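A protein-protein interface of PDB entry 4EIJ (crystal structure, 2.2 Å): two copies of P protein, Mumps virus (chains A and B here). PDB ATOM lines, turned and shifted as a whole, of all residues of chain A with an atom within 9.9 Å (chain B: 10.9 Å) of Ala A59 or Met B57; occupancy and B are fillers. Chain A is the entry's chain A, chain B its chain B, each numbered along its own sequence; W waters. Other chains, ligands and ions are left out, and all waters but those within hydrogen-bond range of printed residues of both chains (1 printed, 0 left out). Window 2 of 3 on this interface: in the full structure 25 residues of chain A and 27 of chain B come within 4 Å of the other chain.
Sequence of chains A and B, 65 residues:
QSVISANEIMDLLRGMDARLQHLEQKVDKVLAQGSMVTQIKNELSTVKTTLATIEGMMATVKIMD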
ATOM      1  N   LEU A  51     -24.763 -11.925  36.365  1.00  0.00           N
ATOM      2  CA  LEU A  51     -25.054 -11.428  35.021  1.00  0.00           C
ATOM      3  C   LEU A  51     -26.255 -10.477  35.008  1.00  0.00           C
ATOM      4  O   LEU A  51     -26.237  -9.467  34.319  1.00  0.00           O
ATOM      5  CB  LEU A  51     -25.275 -12.565  34.024  1.00  0.00           C
ATOM      6  CG  LEU A  51     -24.008 -13.116  33.374  1.00  0.00           C
ATOM      7  CD1 LEU A  51     -24.328 -14.293  32.474  1.00  0.00           C
ATOM      8  CD2 LEU A  51     -23.310 -12.013  32.593  1.00  0.00           C
ATOM      9  N   ALA A  52     -27.299 -10.824  35.755  1.00  0.00           N
ATOM     10  CA  ALA A  52     -28.510 -10.018  35.772  1.00  0.00           C
ATOM     11  C   ALA A  52     -28.186  -8.666  36.407  1.00  0.00           C
ATOM     12  O   ALA A  52     -28.704  -7.633  36.001  1.00  0.00           O
ATOM     13  CB  ALA A  52     -29.610 -10.722  36.541  1.00  0.00           C
ATOM     14  N   THR A  53     -27.314  -8.701  37.408  1.00  0.00           N
ATOM     15  CA  THR A  53     -26.869  -7.502  38.090  1.00  0.00           C
ATOM     16  C   THR A  53     -26.111  -6.614  37.109  1.00  0.00           C
ATOM     17  O   THR A  53     -26.363  -5.419  37.034  1.00  0.00           O
ATOM     18  CB  THR A  53     -25.962  -7.834  39.303  1.00  0.00           C
ATOM     19  OG1 THR A  53     -26.711  -8.576  40.275  1.00  0.00           O
ATOM     20  CG2 THR A  53     -25.445  -6.561  39.953  1.00  0.00           C
ATOM     21  N   ILE A  54     -25.196  -7.217  36.351  1.00  0.00           N
ATOM     22  CA  ILE A  54     -24.437  -6.503  35.324  1.00  0.00           C
ATOM     23  C   ILE A  54     -25.372  -5.851  34.296  1.00  0.00           C
ATOM     24  O   ILE A  54     -25.222  -4.679  33.971  1.00  0.00           O
ATOM     25  CB  ILE A  54     -23.389  -7.424  34.658  1.00  0.00           C
ATOM     26  CG1 ILE A  54     -22.299  -7.784  35.678  1.00  0.00           C
ATOM     27  CG2 ILE A  54     -22.749  -6.753  33.461  1.00  0.00           C
ATOM     28  CD1 ILE A  54     -21.317  -8.831  35.197  1.00  0.00           C
ATOM     29  N   GLU A  55     -26.360  -6.600  33.814  1.00  0.00           N
ATOM     30  CA  GLU A  55     -27.369  -6.005  32.953  1.00  0.00           C
ATOM     31  C   GLU A  55     -27.940  -4.711  33.556  1.00  0.00           C
ATOM     32  O   GLU A  55     -28.109  -3.721  32.854  1.00  0.00           O
ATOM     33  CB  GLU A  55     -28.502  -6.987  32.678  1.00  0.00           C
ATOM     34  CG  GLU A  55     -29.641  -6.370  31.868  1.00  0.00           C
ATOM     35  CD  GLU A  55     -30.811  -7.325  31.691  1.00  0.00           C
ATOM     36  OE1 GLU A  55     -31.971  -6.867  31.738  1.00  0.00           O
ATOM     37  OE2 GLU A  55     -30.569  -8.539  31.511  1.00  0.00           O
ATOM     38  N   GLY A  56     -28.240  -4.729  34.851  1.00  0.00           N
ATOM     39  CA  GLY A  56     -28.843  -3.585  35.509  1.00  0.00           C
ATOM     40  C   GLY A  56     -27.884  -2.407  35.640  1.00  0.00           C
ATOM     41  O   GLY A  56     -28.279  -1.252  35.453  1.00  0.00           O
ATOM     42  N   MET A  57     -26.631  -2.707  35.974  1.00  0.00           N
ATOM     43  CA  MET A  57     -25.572  -1.705  36.042  1.00  0.00           C
ATOM     44  C   MET A  57     -25.350  -1.001  34.712  1.00  0.00           C
ATOM     45  O   MET A  57     -25.065   0.188  34.684  1.00  0.00           O
ATOM     46  CB  MET A  57     -24.257  -2.334  36.494  1.00  0.00           C
ATOM     47  CG  MET A  57     -24.273  -2.813  37.931  1.00  0.00           C
ATOM     48  SD  MET A  57     -22.757  -3.672  38.405  1.00  0.00           S
ATOM     49  CE  MET A  57     -21.535  -2.407  38.088  1.00  0.00           C
ATOM     50  N   MET A  58     -25.460  -1.745  33.617  1.00  0.00           N
ATOM     51  CA  MET A  58     -25.262  -1.179  32.288  1.00  0.00           C
ATOM     52  C   MET A  58     -26.413  -0.286  31.855  1.00  0.00           C
ATOM     53  O   MET A  58     -26.202   0.683  31.140  1.00  0.00           O
ATOM     54  CB  MET A  58     -25.086  -2.293  31.255  1.00  0.00           C
ATOM     55  CG  MET A  58     -23.790  -3.066  31.407  1.00  0.00           C
ATOM     56  SD  MET A  58     -23.703  -4.460  30.284  1.00  0.00           S
ATOM     57  CE  MET A  58     -23.665  -3.618  28.706  1.00  0.00           C
ATOM     58  N   ALA A  59     -27.632  -0.639  32.253  1.00  0.00           N
ATOM     59  CA  ALA A  59     -28.812   0.116  31.842  1.00  0.00           C
ATOM     60  C   ALA A  59     -28.811   1.518  32.464  1.00  0.00           C
ATOM     61  O   ALA A  59     -28.371   1.704  33.594  1.00  0.00           O
ATOM     62  CB  ALA A  59     -30.084  -0.630  32.224  1.00  0.00           C
ATOM     63  N   THR A  60     -29.298   2.496  31.712  1.00  0.00           N
ATOM     64  CA  THR A  60     -29.474   3.854  32.219  1.00  0.00           C
ATOM     65  C   THR A  60     -30.843   3.951  32.860  1.00  0.00           C
ATOM     66  O   THR A  60     -31.853   3.696  32.217  1.00  0.00           O
ATOM     67  CB  THR A  60     -29.408   4.886  31.078  1.00  0.00           C
ATOM     68  OG1 THR A  60     -28.133   4.805  30.432  1.00  0.00           O
ATOM     69  CG2 THR A  60     -29.634   6.323  31.600  1.00  0.00           C
ATOM     70  N   VAL A  61     -30.880   4.325  34.127  1.00  0.00           N
ATOM     71  CA  VAL A  61     -32.150   4.458  34.832  1.00  0.00           C
ATOM     72  C   VAL A  61     -32.425   5.900  35.216  1.00  0.00           C
ATOM     73  O   VAL A  61     -31.591   6.539  35.855  1.00  0.00           O
ATOM     74  CB  VAL A  61     -32.173   3.598  36.105  1.00  0.00           C
ATOM     75  CG1 VAL A  61     -33.326   4.008  37.012  1.00  0.00           C
ATOM     76  CG2 VAL A  61     -32.271   2.121  35.736  1.00  0.00           C
ATOM     77  N   LYS A  62     -33.601   6.388  34.821  1.00  0.00           N
ATOM     78  CA  LYS A  62     -34.075   7.724  35.167  1.00  0.00           C
ATOM     79  C   LYS A  62     -35.062   7.665  36.328  1.00  0.00           C
ATOM     80  O   LYS A  62     -36.096   7.000  36.241  1.00  0.00           O
ATOM     81  CB  LYS A  62     -34.745   8.385  33.954  1.00  0.00           C
ATOM     82  CG  LYS A  62     -35.208   7.408  32.863  1.00  0.00           C
ATOM     83  CD  LYS A  62     -36.658   6.940  33.013  1.00  0.00           C
ATOM     84  CE  LYS A  62     -37.064   6.077  31.815  1.00  0.00           C
ATOM     85  NZ  LYS A  62     -38.533   5.891  31.621  1.00  0.00           N
ATOM     86  N   THR B  49     -30.894 -15.917  28.484  1.00  0.00           N
ATOM     87  CA  THR B  49     -31.755 -14.781  28.193  1.00  0.00           C
ATOM     88  C   THR B  49     -31.062 -13.491  28.609  1.00  0.00           C
ATOM     89  O   THR B  49     -31.089 -12.495  27.892  1.00  0.00           O
ATOM     90  CB  THR B  49     -33.118 -14.914  28.883  1.00  0.00           C
ATOM     91  OG1 THR B  49     -33.885 -15.900  28.200  1.00  0.00           O
ATOM     92  CG2 THR B  49     -33.873 -13.604  28.835  1.00  0.00           C
ATOM     93  N   THR B  50     -30.411 -13.533  29.761  1.00  0.00           N
ATOM     94  CA  THR B  50     -29.646 -12.396  30.240  1.00  0.00           C
ATOM     95  C   THR B  50     -28.495 -12.044  29.284  1.00  0.00           C
ATOM     96  O   THR B  50     -28.276 -10.868  28.992  1.00  0.00           O
ATOM     97  CB  THR B  50     -29.101 -12.663  31.655  1.00  0.00           C
ATOM     98  OG1 THR B  50     -30.188 -13.000  32.527  1.00  0.00           O
ATOM     99  CG2 THR B  50     -28.366 -11.428  32.197  1.00  0.00           C
ATOM    100  N   LEU B  51     -27.767 -13.049  28.787  1.00  0.00           N
ATOM    101  CA  LEU B  51     -26.666 -12.770  27.851  1.00  0.00           C
ATOM    102  C   LEU B  51     -27.178 -12.117  26.586  1.00  0.00           C
ATOM    103  O   LEU B  51     -26.537 -11.212  26.041  1.00  0.00           O
ATOM    104  CB  LEU B  51     -25.918 -14.045  27.456  1.00  0.00           C
ATOM    105  CG  LEU B  51     -24.892 -14.620  28.424  1.00  0.00           C
ATOM    106  CD1 LEU B  51     -24.421 -15.973  27.908  1.00  0.00           C
ATOM    107  CD2 LEU B  51     -23.725 -13.655  28.610  1.00  0.00           C
ATOM    108  N   ALA B  52     -28.326 -12.597  26.108  1.00  0.00           N
ATOM    109  CA  ALA B  52     -28.915 -12.066  24.885  1.00  0.00           C
ATOM    110  C   ALA B  52     -29.316 -10.596  25.060  1.00  0.00           C
ATOM    111  O   ALA B  52     -29.213  -9.808  24.129  1.00  0.00           O
ATOM    112  CB  ALA B  52     -30.109 -12.899  24.463  1.00  0.00           C
ATOM    113  N   THR B  53     -29.783 -10.233  26.249  1.00  0.00           N
ATOM    114  CA  THR B  53     -30.157  -8.849  26.498  1.00  0.00           C
ATOM    115  C   THR B  53     -28.893  -7.988  26.502  1.00  0.00           C
ATOM    116  O   THR B  53     -28.825  -6.969  25.825  1.00  0.00           O
ATOM    117  CB  THR B  53     -30.925  -8.693  27.822  1.00  0.00           C
ATOM    118  OG1 THR B  53     -32.184  -9.365  27.716  1.00  0.00           O
ATOM    119  CG2 THR B  53     -31.178  -7.201  28.141  1.00  0.00           C
ATOM    120  N   ILE B  54     -27.881  -8.434  27.238  1.00  0.00           N
ATOM    121  CA  ILE B  54     -26.595  -7.745  27.263  1.00  0.00           C
ATOM    122  C   ILE B  54     -26.002  -7.611  25.854  1.00  0.00           C
ATOM    123  O   ILE B  54     -25.445  -6.576  25.517  1.00  0.00           O
ATOM    124  CB  ILE B  54     -25.595  -8.424  28.228  1.00  0.00           C
ATOM    125  CG1 ILE B  54     -26.175  -8.430  29.649  1.00  0.00           C
ATOM    126  CG2 ILE B  54     -24.257  -7.659  28.219  1.00  0.00           C
ATOM    127  CD1 ILE B  54     -25.396  -9.247  30.646  1.00  0.00           C
ATOM    128  N   GLU B  55     -26.154  -8.646  25.031  1.00  0.00           N
ATOM    129  CA  GLU B  55     -25.723  -8.576  23.637  1.00  0.00           C
ATOM    130  C   GLU B  55     -26.476  -7.512  22.842  1.00  0.00           C
ATOM    131  O   GLU B  55     -25.863  -6.765  22.089  1.00  0.00           O
ATOM    132  CB  GLU B  55     -25.797  -9.948  22.959  1.00  0.00           C
ATOM    133  CG  GLU B  55     -24.643 -10.840  23.377  1.00  0.00           C
ATOM    134  CD  GLU B  55     -24.820 -12.300  22.982  1.00  0.00           C
ATOM    135  OE1 GLU B  55     -25.938 -12.687  22.588  1.00  0.00           O
ATOM    136  OE2 GLU B  55     -23.829 -13.058  23.072  1.00  0.00           O
ATOM    137  N   GLY B  56     -27.791  -7.442  23.017  1.00  0.00           N
ATOM    138  CA  GLY B  56     -28.578  -6.375  22.414  1.00  0.00           C
ATOM    139  C   GLY B  56     -28.076  -5.000  22.847  1.00  0.00           C
ATOM    140  O   GLY B  56     -27.940  -4.093  22.030  1.00  0.00           O
ATOM    141  N   MET B  57     -27.788  -4.852  24.136  1.00  0.00           N
ATOM    142  CA  MET B  57     -27.226  -3.612  24.658  1.00  0.00           C
ATOM    143  C   MET B  57     -25.925  -3.265  23.946  1.00  0.00           C
ATOM    144  O   MET B  57     -25.753  -2.143  23.460  1.00  0.00           O
ATOM    145  CB  MET B  57     -26.966  -3.719  26.166  1.00  0.00           C
ATOM    146  CG  MET B  57     -28.220  -3.753  27.030  1.00  0.00           C
ATOM    147  SD  MET B  57     -27.856  -3.978  28.784  1.00  0.00           S
ATOM    148  CE  MET B  57     -29.346  -3.320  29.526  1.00  0.00           C
ATOM    149  N   MET B  58     -25.007  -4.227  23.883  1.00  0.00           N
ATOM    150  CA  MET B  58     -23.691  -3.965  23.308  1.00  0.00           C
ATOM    151  C   MET B  58     -23.757  -3.658  21.818  1.00  0.00           C
ATOM    152  O   MET B  58     -22.884  -2.979  21.283  1.00  0.00           O
ATOM    153  CB  MET B  58     -22.735  -5.131  23.576  1.00  0.00           C
ATOM    154  CG  MET B  58     -22.373  -5.290  25.036  1.00  0.00           C
ATOM    155  SD  MET B  58     -21.771  -3.721  25.704  1.00  0.00           S
ATOM    156  CE  MET B  58     -20.352  -3.422  24.648  1.00  0.00           C
ATOM    157  N   ALA B  59     -24.797  -4.152  21.155  1.00  0.00           N
ATOM    158  CA  ALA B  59     -24.926  -3.982  19.713  1.00  0.00           C
ATOM    159  C   ALA B  59     -25.354  -2.565  19.366  1.00  0.00           C
ATOM    160  O   ALA B  59     -25.153  -2.110  18.247  1.00  0.00           O
ATOM    161  CB  ALA B  59     -25.926  -4.990  19.141  1.00  0.00           C
ATOM    162  N   THR B  60     -25.968  -1.894  20.335  1.00  0.00           N
ATOM    163  CA  THR B  60     -26.464  -0.538  20.164  1.00  0.00           C
ATOM    164  C   THR B  60     -25.721   0.399  21.117  1.00  0.00           C
ATOM    165  O   THR B  60     -26.322   1.269  21.752  1.00  0.00           O
ATOM    166  CB  THR B  60     -27.979  -0.462  20.451  1.00  0.00           C
ATOM    167  OG1 THR B  60     -28.252  -1.095  21.702  1.00  0.00           O
ATOM    168  CG2 THR B  60     -28.782  -1.163  19.354  1.00  0.00           C
ATOM    169  N   VAL B  61     -24.408   0.204  21.207  1.00  0.00           N
ATOM    170  CA  VAL B  61     -23.553   1.007  22.071  1.00  0.00           C
ATOM    171  C   VAL B  61     -23.689   0.575  23.519  1.00  0.00           C
ATOM    172  O   VAL B  61     -22.701   0.218  24.157  1.00  0.00           O
ATOM    173  CB  VAL B  61     -23.862   2.511  21.949  1.00  0.00           C
ATOM    174  CG1 VAL B  61     -23.723   3.186  23.296  1.00  0.00           C
ATOM    175  CG2 VAL B  61     -22.964   3.150  20.914  1.00  0.00           C
HETATM  176  O   HOH W   1     -33.112  -9.874  30.386  1.00  0.00           O
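O of Thr B49 sits at hydrogen-bond distance from OG1 of Thr B53, 3.3 Å away. O of Met B57 sits at hydrogen-bond distance from OG1 of Thr B60.
Water W1 bridges OG1 of Thr B53 (2.9 Å) and OE2 of Glu A55 (3.1 Å).
Of chain B, only Thr B50 (3.7 Å), Thr B53 (3.6 Å) and Met B57 (3.6 Å) come within 4 Å of Glu A55. Gly A56 touches none of the printed residues of chain B. No residue of chain B comes within 4 Å of Val A61. Of the printed residues of chain A, Thr B50 touches Leu A51 (3.6 Å), Ala A52 (3.8 Å) and Glu A55 (3.7 Å). Of the printed residues of chain A, Leu B51 touches Leu A51 (3.96 Å). Printed residues of chain A within 4 Å of Thr B53: Glu A55 (3.6 Å). Printed residues of chain A within 4 Å of Ile B54: Leu A51 (3.8 Å) and Met A58 (3.8 Å). Printed residues of chain A within 4 Å of Met B57: Glu A55 and Ala A59. Met B58 touches just one residue of chain A: Met A58 (3.6 Å).
Leu A51 touches Ile B54, but with the chains exchanged Ile A54 does not touch Leu B51 (8.5 Å). Glu A55 touches Met B57, but with the chains exchanged Met A57 does not touch Glu B55 (12.4 Å). Met A58 touches Ile B54, but with the chains exchanged Ile A54 does not touch Met B58 (8.4 Å). Met B58 touches its own counterpart, Met A58. Positions printed for both chains: 51, 52, 53, 54, 55, 56, 57, 58, 59, 60 and 61.
Hydrophobic or aromatic side chains of chain A within 4 Å of the printed part of chain B: Leu A51, Met A58 and Ala A59. Hydrophobic or aromatic side chains of chain B that line the printed part of chain A: Leu B51, Ile B54, Met B57 and Met B58. Among the printed residues, no Asp or Glu carboxylate lies within 4 Å of a Lys or Arg side-chain nitrogen of the other chain.
Among the printed residues, pairs that only touch across the chains: Met A58 with Met B58 (3.6 Å), Glu A55 with Thr B53 (3.6 Å), Glu A55 with Met B57 (3.6 Å), Leu A51 with Thr B50 (3.6 Å), Glu A55 with Thr B50 (3.7 Å), Ala A52 with Thr B50 (3.8 Å), Leu A51 with Ile B54 (3.8 Å), Met A58 with Ile B54 (3.8 Å), Ala A59 with Met B57 (3.9 Å) and Leu A51 with Leu B51 (3.96 Å).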
